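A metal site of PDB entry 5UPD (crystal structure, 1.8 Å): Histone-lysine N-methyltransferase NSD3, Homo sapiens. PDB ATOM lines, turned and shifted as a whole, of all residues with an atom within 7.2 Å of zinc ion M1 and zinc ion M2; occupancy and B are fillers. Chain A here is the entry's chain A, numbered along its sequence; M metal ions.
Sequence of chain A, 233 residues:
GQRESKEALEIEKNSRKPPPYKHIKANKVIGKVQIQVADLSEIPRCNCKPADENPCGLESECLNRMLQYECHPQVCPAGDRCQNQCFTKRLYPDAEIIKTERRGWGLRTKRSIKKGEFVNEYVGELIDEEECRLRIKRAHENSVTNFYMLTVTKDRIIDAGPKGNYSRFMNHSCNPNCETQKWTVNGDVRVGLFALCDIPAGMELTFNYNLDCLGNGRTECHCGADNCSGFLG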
ATOM      1  N   ARG A  45      -4.355  -1.170  -9.258  1.00  0.00           N
ATOM      2  CA  ARG A  45      -4.753  -2.351 -10.000  1.00  0.00           C
ATOM      3  C   ARG A  45      -4.395  -3.596  -9.171  1.00  0.00           C
ATOM      4  O   ARG A  45      -3.301  -3.722  -8.694  1.00  0.00           O
ATOM      5  CB  ARG A  45      -4.033  -2.378 -11.355  1.00  0.00           C
ATOM      6  CG  ARG A  45      -4.231  -3.640 -12.192  1.00  0.00           C
ATOM      7  CD  ARG A  45      -3.531  -3.599 -13.563  1.00  0.00           C
ATOM      8  NE  ARG A  45      -3.975  -2.437 -14.348  1.00  0.00           N
ATOM      9  CZ  ARG A  45      -3.232  -1.382 -14.705  1.00  0.00           C
ATOM     10  NH1 ARG A  45      -1.928  -1.296 -14.403  1.00  0.00           N
ATOM     11  NH2 ARG A  45      -3.796  -0.387 -15.391  1.00  0.00           N
ATOM     12  N   CYS A  46      -5.345  -4.493  -9.010  1.00  0.00           N
ATOM     13  CA  CYS A  46      -5.118  -5.760  -8.343  1.00  0.00           C
ATOM     14  C   CYS A  46      -4.524  -6.804  -9.335  1.00  0.00           C
ATOM     15  O   CYS A  46      -4.401  -6.545 -10.534  1.00  0.00           O
ATOM     16  CB  CYS A  46      -6.429  -6.265  -7.802  1.00  0.00           C
ATOM     17  SG  CYS A  46      -7.604  -6.875  -9.036  1.00  0.00           S
ATOM     18  N   ASN A  47      -4.251  -7.999  -8.821  1.00  0.00           N
ATOM     19  CA  ASN A  47      -3.616  -9.068  -9.597  1.00  0.00           C
ATOM     20  C   ASN A  47      -4.594 -10.215  -9.912  1.00  0.00           C
ATOM     21  O   ASN A  47      -4.183 -11.272 -10.381  1.00  0.00           O
ATOM     22  CB  ASN A  47      -2.369  -9.615  -8.849  1.00  0.00           C
ATOM     23  CG  ASN A  47      -1.234  -8.563  -8.690  1.00  0.00           C
ATOM     24  OD1 ASN A  47      -1.150  -7.568  -9.420  1.00  0.00           O
ATOM     25  ND2 ASN A  47      -0.326  -8.817  -7.745  1.00  0.00           N
ATOM     26  N   CYS A  48      -5.894  -9.995  -9.673  1.00  0.00           N
ATOM     27  CA  CYS A  48      -6.937 -10.977  -9.991  1.00  0.00           C
ATOM     28  C   CYS A  48      -7.083 -11.228 -11.509  1.00  0.00           C
ATOM     29  O   CYS A  48      -6.675 -10.412 -12.310  1.00  0.00           O
ATOM     30  CB  CYS A  48      -8.292 -10.570  -9.406  1.00  0.00           C
ATOM     31  SG  CYS A  48      -8.341 -10.229  -7.614  1.00  0.00           S
ATOM     32  N   LYS A  49      -7.694 -12.352 -11.880  1.00  0.00           N
ATOM     33  CA  LYS A  49      -7.746 -12.758 -13.296  1.00  0.00           C
ATOM     34  C   LYS A  49      -9.166 -13.000 -13.757  1.00  0.00           C
ATOM     35  O   LYS A  49     -10.022 -13.464 -12.981  1.00  0.00           O
ATOM     36  CB  LYS A  49      -6.852 -13.997 -13.548  1.00  0.00           C
ATOM     37  CG  LYS A  49      -5.375 -13.645 -13.694  1.00  0.00           C
ATOM     38  CD  LYS A  49      -4.444 -14.804 -13.348  1.00  0.00           C
ATOM     39  CE  LYS A  49      -2.989 -14.443 -13.627  1.00  0.00           C
ATOM     40  NZ  LYS A  49      -2.096 -15.632 -13.481  1.00  0.00           N
ATOM     41  N   ASP A  52     -10.437 -16.376 -12.868  1.00  0.00           N
ATOM     42  CA  ASP A  52     -10.714 -16.810 -11.484  1.00  0.00           C
ATOM     43  C   ASP A  52     -12.216 -16.994 -11.350  1.00  0.00           C
ATOM     44  O   ASP A  52     -12.984 -16.421 -12.119  1.00  0.00           O
ATOM     45  CB  ASP A  52     -10.244 -15.777 -10.442  1.00  0.00           C
ATOM     46  CG  ASP A  52      -8.726 -15.561 -10.449  1.00  0.00           C
ATOM     47  OD1 ASP A  52      -7.991 -16.281 -11.169  1.00  0.00           O
ATOM     48  OD2 ASP A  52      -8.252 -14.650  -9.704  1.00  0.00           O
ATOM     49  N   PRO A  55     -14.090 -13.199  -9.469  1.00  0.00           N
ATOM     50  CA  PRO A  55     -12.950 -12.286  -9.453  1.00  0.00           C
ATOM     51  C   PRO A  55     -13.223 -11.011  -8.580  1.00  0.00           C
ATOM     52  O   PRO A  55     -14.273 -10.425  -8.687  1.00  0.00           O
ATOM     53  CB  PRO A  55     -12.740 -11.938 -10.933  1.00  0.00           C
ATOM     54  CG  PRO A  55     -13.966 -12.402 -11.639  1.00  0.00           C
ATOM     55  CD  PRO A  55     -14.577 -13.486 -10.832  1.00  0.00           C
ATOM     56  N   CYS A  56     -12.247 -10.682  -7.740  1.00  0.00           N
ATOM     57  CA  CYS A  56     -12.315  -9.579  -6.776  1.00  0.00           C
ATOM     58  C   CYS A  56     -13.441  -9.713  -5.749  1.00  0.00           C
ATOM     59  O   CYS A  56     -13.833  -8.737  -5.148  1.00  0.00           O
ATOM     60  CB  CYS A  56     -12.345  -8.222  -7.489  1.00  0.00           C
ATOM     61  SG  CYS A  56     -11.023  -8.049  -8.738  1.00  0.00           S
ATOM     62  N   GLY A  57     -13.875 -10.945  -5.485  1.00  0.00           N
ATOM     63  CA  GLY A  57     -14.998 -11.232  -4.591  1.00  0.00           C
ATOM     64  C   GLY A  57     -14.596 -11.331  -3.132  1.00  0.00           C
ATOM     65  O   GLY A  57     -13.407 -11.272  -2.758  1.00  0.00           O
ATOM     66  N   SER A  60     -11.863 -13.970  -2.341  1.00  0.00           N
ATOM     67  CA  SER A  60     -10.588 -13.846  -3.074  1.00  0.00           C
ATOM     68  C   SER A  60      -9.452 -13.209  -2.279  1.00  0.00           C
ATOM     69  O   SER A  60      -9.669 -12.644  -1.228  1.00  0.00           O
ATOM     70  CB  SER A  60     -10.819 -13.021  -4.345  1.00  0.00           C
ATOM     71  OG  SER A  60     -10.979 -11.646  -4.044  1.00  0.00           O
ATOM     72  N   GLU A  61      -8.233 -13.288  -2.812  1.00  0.00           N
ATOM     73  CA  GLU A  61      -7.102 -12.610  -2.200  1.00  0.00           C
ATOM     74  C   GLU A  61      -6.943 -11.203  -2.798  1.00  0.00           C
ATOM     75  O   GLU A  61      -5.855 -10.654  -2.772  1.00  0.00           O
ATOM     76  CB  GLU A  61      -5.802 -13.405  -2.445  1.00  0.00           C
ATOM     77  N   CYS A  62      -8.024 -10.601  -3.326  1.00  0.00           N
ATOM     78  CA  CYS A  62      -7.882  -9.368  -4.103  1.00  0.00           C
ATOM     79  C   CYS A  62      -7.140  -8.350  -3.266  1.00  0.00           C
ATOM     80  O   CYS A  62      -7.548  -8.071  -2.143  1.00  0.00           O
ATOM     81  CB  CYS A  62      -9.248  -8.824  -4.476  1.00  0.00           C
ATOM     82  SG  CYS A  62      -9.182  -7.252  -5.388  1.00  0.00           S
ATOM     83  N   LEU A  63      -6.035  -7.827  -3.807  1.00  0.00           N
ATOM     84  CA  LEU A  63      -5.237  -6.819  -3.113  1.00  0.00           C
ATOM     85  C   LEU A  63      -6.017  -5.538  -2.910  1.00  0.00           C
ATOM     86  O   LEU A  63      -5.763  -4.870  -1.948  1.00  0.00           O
ATOM     87  CB  LEU A  63      -3.944  -6.493  -3.857  1.00  0.00           C
ATOM     88  CG  LEU A  63      -2.888  -7.600  -4.073  1.00  0.00           C
ATOM     89  CD1 LEU A  63      -1.981  -7.190  -5.215  1.00  0.00           C
ATOM     90  CD2 LEU A  63      -2.070  -7.896  -2.804  1.00  0.00           C
ATOM     91  N   ASN A  64      -6.943  -5.193  -3.800  1.00  0.00           N
ATOM     92  CA  ASN A  64      -7.705  -3.943  -3.644  1.00  0.00           C
ATOM     93  C   ASN A  64      -8.682  -4.130  -2.486  1.00  0.00           C
ATOM     94  O   ASN A  64      -8.735  -3.307  -1.594  1.00  0.00           O
ATOM     95  CB  ASN A  64      -8.439  -3.516  -4.914  1.00  0.00           C
ATOM     96  CG  ASN A  64      -7.537  -2.808  -5.910  1.00  0.00           C
ATOM     97  OD1 ASN A  64      -6.396  -2.453  -5.593  1.00  0.00           O
ATOM     98  ND2 ASN A  64      -8.052  -2.573  -7.092  1.00  0.00           N
ATOM     99  N   ARG A  65      -9.462  -5.194  -2.506  1.00  0.00           N
ATOM    100  CA  ARG A  65     -10.337  -5.528  -1.359  1.00  0.00           C
ATOM    101  C   ARG A  65      -9.651  -5.488  -0.036  1.00  0.00           C
ATOM    102  O   ARG A  65     -10.252  -4.986   0.932  1.00  0.00           O
ATOM    103  CB  ARG A  65     -10.856  -6.942  -1.446  1.00  0.00           C
ATOM    104  CG  ARG A  65     -12.033  -7.107  -2.325  1.00  0.00           C
ATOM    105  CD  ARG A  65     -12.964  -8.130  -1.757  1.00  0.00           C
ATOM    106  NE  ARG A  65     -14.177  -7.945  -2.512  1.00  0.00           N
ATOM    107  CZ  ARG A  65     -15.289  -7.403  -2.053  1.00  0.00           C
ATOM    108  NH1 ARG A  65     -15.421  -7.011  -0.799  1.00  0.00           N
ATOM    109  NH2 ARG A  65     -16.303  -7.278  -2.894  1.00  0.00           N
ATOM    110  N   GLU A  70     -11.985   0.136  -3.786  1.00  0.00           N
ATOM    111  CA  GLU A  70     -12.858  -0.326  -4.862  1.00  0.00           C
ATOM    112  C   GLU A  70     -12.080  -0.335  -6.193  1.00  0.00           C
ATOM    113  O   GLU A  70     -11.336   0.591  -6.495  1.00  0.00           O
ATOM    114  CB  GLU A  70     -14.101   0.590  -4.965  1.00  0.00           C
ATOM    115  CG  GLU A  70     -15.034   0.272  -6.097  1.00  0.00           C
ATOM    116  CD  GLU A  70     -16.544   0.426  -5.785  1.00  0.00           C
ATOM    117  OE1 GLU A  70     -17.002  -0.042  -4.725  1.00  0.00           O
ATOM    118  OE2 GLU A  70     -17.276   0.984  -6.648  1.00  0.00           O
ATOM    119  N   CYS A  71     -12.268  -1.389  -6.976  1.00  0.00           N
ATOM    120  CA  CYS A  71     -11.737  -1.462  -8.352  1.00  0.00           C
ATOM    121  C   CYS A  71     -12.491  -0.518  -9.260  1.00  0.00           C
ATOM    122  O   CYS A  71     -13.659  -0.191  -9.038  1.00  0.00           O
ATOM    123  CB  CYS A  71     -11.865  -2.903  -8.901  1.00  0.00           C
ATOM    124  SG  CYS A  71     -10.924  -4.166  -8.084  1.00  0.00           S
ATOM    125  N   HIS A  72     -11.803   0.014 -10.250  1.00  0.00           N
ATOM    126  CA  HIS A  72     -12.417   0.833 -11.265  1.00  0.00           C
ATOM    127  C   HIS A  72     -12.499  -0.085 -12.496  1.00  0.00           C
ATOM    128  O   HIS A  72     -11.504  -0.705 -12.835  1.00  0.00           O
ATOM    129  CB  HIS A  72     -11.522   2.018 -11.593  1.00  0.00           C
ATOM    130  CG  HIS A  72     -12.165   3.004 -12.505  1.00  0.00           C
ATOM    131  ND1 HIS A  72     -12.483   2.693 -13.820  1.00  0.00           N
ATOM    132  CD2 HIS A  72     -12.511   4.300 -12.315  1.00  0.00           C
ATOM    133  CE1 HIS A  72     -13.046   3.754 -14.379  1.00  0.00           C
ATOM    134  NE2 HIS A  72     -13.061   4.753 -13.495  1.00  0.00           N
ATOM    135  N   PRO A  73     -13.665  -0.165 -13.173  1.00  0.00           N
ATOM    136  CA  PRO A  73     -13.854  -1.103 -14.293  1.00  0.00           C
ATOM    137  C   PRO A  73     -12.849  -0.916 -15.469  1.00  0.00           C
ATOM    138  O   PRO A  73     -12.424  -1.907 -16.050  1.00  0.00           O
ATOM    139  CB  PRO A  73     -15.302  -0.856 -14.726  1.00  0.00           C
ATOM    140  CG  PRO A  73     -15.629   0.500 -14.244  1.00  0.00           C
ATOM    141  CD  PRO A  73     -14.886   0.636 -12.949  1.00  0.00           C
ATOM    142  N   VAL A  75      -9.726  -0.172 -15.079  1.00  0.00           N
ATOM    143  CA  VAL A  75      -8.400  -0.533 -14.588  1.00  0.00           C
ATOM    144  C   VAL A  75      -8.318  -2.025 -14.259  1.00  0.00           C
ATOM    145  O   VAL A  75      -7.281  -2.631 -14.466  1.00  0.00           O
ATOM    146  CB  VAL A  75      -8.041   0.313 -13.333  1.00  0.00           C
ATOM    147  CG1 VAL A  75      -6.711  -0.110 -12.706  1.00  0.00           C
ATOM    148  CG2 VAL A  75      -7.955   1.784 -13.697  1.00  0.00           C
ATOM    149  N   CYS A  76      -9.389  -2.615 -13.765  1.00  0.00           N
ATOM    150  CA  CYS A  76      -9.327  -3.946 -13.222  1.00  0.00           C
ATOM    151  C   CYS A  76      -9.066  -4.969 -14.305  1.00  0.00           C
ATOM    152  O   CYS A  76      -9.761  -4.949 -15.318  1.00  0.00           O
ATOM    153  CB  CYS A  76     -10.642  -4.319 -12.549  1.00  0.00           C
ATOM    154  SG  CYS A  76     -10.500  -5.868 -11.697  1.00  0.00           S
ATOM    155  N   PRO A  77      -8.125  -5.911 -14.071  1.00  0.00           N
ATOM    156  CA  PRO A  77      -7.887  -6.948 -15.073  1.00  0.00           C
ATOM    157  C   PRO A  77      -9.072  -7.891 -15.280  1.00  0.00           C
ATOM    158  O   PRO A  77      -9.180  -8.485 -16.368  1.00  0.00           O
ATOM    159  CB  PRO A  77      -6.670  -7.726 -14.533  1.00  0.00           C
ATOM    160  CG  PRO A  77      -6.093  -6.856 -13.462  1.00  0.00           C
ATOM    161  CD  PRO A  77      -7.254  -6.120 -12.903  1.00  0.00           C
ATOM    162  N   ALA A  78      -9.969  -8.010 -14.289  1.00  0.00           N
ATOM    163  CA  ALA A  78     -11.195  -8.783 -14.484  1.00  0.00           C
ATOM    164  C   ALA A  78     -12.302  -8.023 -15.213  1.00  0.00           C
ATOM    165  O   ALA A  78     -13.386  -8.559 -15.426  1.00  0.00           O
ATOM    166  CB  ALA A  78     -11.710  -9.308 -13.149  1.00  0.00           C
ATOM    167  N   GLY A  79     -12.063  -6.762 -15.565  1.00  0.00           N
ATOM    168  CA  GLY A  79     -13.039  -5.972 -16.297  1.00  0.00           C
ATOM    169  C   GLY A  79     -14.389  -5.907 -15.585  1.00  0.00           C
ATOM    170  O   GLY A  79     -14.486  -5.359 -14.494  1.00  0.00           O
ATOM    171  N   ARG A  81     -16.501  -8.617 -14.925  1.00  0.00           N
ATOM    172  CA  ARG A  81     -16.724  -9.692 -13.959  1.00  0.00           C
ATOM    173  C   ARG A  81     -16.200  -9.345 -12.552  1.00  0.00           C
ATOM    174  O   ARG A  81     -16.366 -10.119 -11.637  1.00  0.00           O
ATOM    175  CB  ARG A  81     -16.063 -11.006 -14.423  1.00  0.00           C
ATOM    176  CG  ARG A  81     -16.522 -11.491 -15.794  1.00  0.00           C
ATOM    177  CD  ARG A  81     -16.681 -13.007 -15.887  1.00  0.00           C
ATOM    178  NE  ARG A  81     -15.582 -13.774 -15.268  1.00  0.00           N
ATOM    179  CZ  ARG A  81     -15.678 -14.545 -14.167  1.00  0.00           C
ATOM    180  NH1 ARG A  81     -14.607 -15.208 -13.725  1.00  0.00           N
ATOM    181  NH2 ARG A  81     -16.833 -14.676 -13.490  1.00  0.00           N
ATOM    182  N   CYS A  82     -15.538  -8.195 -12.422  1.00  0.00           N
ATOM    183  CA  CYS A  82     -15.005  -7.749 -11.145  1.00  0.00           C
ATOM    184  C   CYS A  82     -16.146  -7.641 -10.116  1.00  0.00           C
ATOM    185  O   CYS A  82     -17.100  -6.910 -10.359  1.00  0.00           O
ATOM    186  CB  CYS A  82     -14.336  -6.386 -11.327  1.00  0.00           C
ATOM    187  SG  CYS A  82     -13.760  -5.587  -9.794  1.00  0.00           S
ATOM    188  N   GLN A  83     -16.017  -8.316  -8.986  1.00  0.00           N
ATOM    189  CA  GLN A  83     -17.020  -8.264  -7.904  1.00  0.00           C
ATOM    190  C   GLN A  83     -16.645  -7.242  -6.802  1.00  0.00           C
ATOM    191  O   GLN A  83     -17.114  -7.357  -5.672  1.00  0.00           O
ATOM    192  CB  GLN A  83     -17.232  -9.664  -7.304  1.00  0.00           C
ATOM    193  CG  GLN A  83     -17.967 -10.610  -8.257  1.00  0.00           C
ATOM    194  CD  GLN A  83     -17.949 -12.063  -7.782  1.00  0.00           C
ATOM    195  OE1 GLN A  83     -17.500 -12.371  -6.661  1.00  0.00           O
ATOM    196  NE2 GLN A  83     -18.431 -12.975  -8.650  1.00  0.00           N
ATOM    197  N   ASN A  84     -15.832  -6.228  -7.160  1.00  0.00           N
ATOM    198  CA  ASN A  84     -15.385  -5.201  -6.202  1.00  0.00           C
ATOM    199  C   ASN A  84     -15.767  -3.862  -6.721  1.00  0.00           C
ATOM    200  O   ASN A  84     -14.943  -2.974  -6.771  1.00  0.00           O
ATOM    201  CB  ASN A  84     -13.909  -5.319  -5.912  1.00  0.00           C
ATOM    202  CG  ASN A  84     -13.415  -4.393  -4.778  1.00  0.00           C
ATOM    203  OD1 ASN A  84     -14.183  -3.998  -3.873  1.00  0.00           O
ATOM    204  ND2 ASN A  84     -12.161  -4.037  -4.851  1.00  0.00           N
ATOM    205  N   GLN A  85     -17.031  -3.723  -7.104  1.00  0.00           N
ATOM    206  CA  GLN A  85     -17.556  -2.440  -7.592  1.00  0.00           C
ATOM    207  C   GLN A  85     -18.825  -2.040  -6.858  1.00  0.00           C
ATOM    208  O   GLN A  85     -19.683  -1.368  -7.429  1.00  0.00           O
ATOM    209  CB  GLN A  85     -17.903  -2.530  -9.066  1.00  0.00           C
ATOM    210  CG  GLN A  85     -16.682  -2.806  -9.966  1.00  0.00           C
ATOM    211  CD  GLN A  85     -17.119  -3.011 -11.408  1.00  0.00           C
ATOM    212  OE1 GLN A  85     -17.485  -2.061 -12.074  1.00  0.00           O
ATOM    213  NE2 GLN A  85     -17.117  -4.267 -11.873  1.00  0.00           N
HETATM  214 ZN    ZN M   1     -11.545  -5.890  -9.564  1.00  0.00          ZN
HETATM  215 ZN    ZN M   2      -9.097  -7.998  -7.644  1.00  0.00          ZN
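Zinc ion M2 is bound by the side-chain sulfur of Cys 56, the side-chain sulfur of Cys 46, the side-chain sulfur of Cys 48 and the side-chain sulfur of Cys 62.
Zinc ion M2 has four donor atoms within binding distance.
Zinc ion M1 is bound by the side-chain sulfur (SG) of Cys 82.
Zinc ion M1 is bound by SG of Cys 71.
Zinc ion M1 is bound by the side-chain sulfur (SG) of Cys 56 (2.4 Å).
Zinc ion M1 is bound by SG of Cys 76, 2.4 Å away.
Zinc ion M1 has four donor atoms within binding distance.
NE of Arg 65 is in hydrogen-bond range of O of Cys 56 (2.8 Å).
The side-chain sulfur (SG) of Cys 82 sits close to the backbone NH (N) of Asn 84 (3.4 Å).
NE2 of Gln 85 lies within hydrogen-bond range of O of Cys 82, 3.0 Å away.
O of Asn 84 sits at hydrogen-bond distance from N of Cys 71, at 3.1 Å.
The side-chain sulfur (SG) of Cys 71 lies close to the side-chain amide nitrogen (ND2) of Asn 64 (3.4 Å).
The backbone NH (N) of Ala 78 sits close to the side-chain sulfur (SG) of Cys 76.
The side-chain sulfur of Cys 62 lies close to the backbone NH of Asn 64.
The backbone NH of Arg 65 sits close to the side-chain sulfur of Cys 62.
Of the 29 residues printed, 4 come within 4 Å of zinc ion M2.
Along chain A the residues within 4 Å of zinc ion M2 span positions 46 to 62.
Of the 29 residues printed, 4 come within 4 Å of zinc ion M1.
The nearest printed residue that does not touch zinc ion M1 is Cys 46 (4.1 Å).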
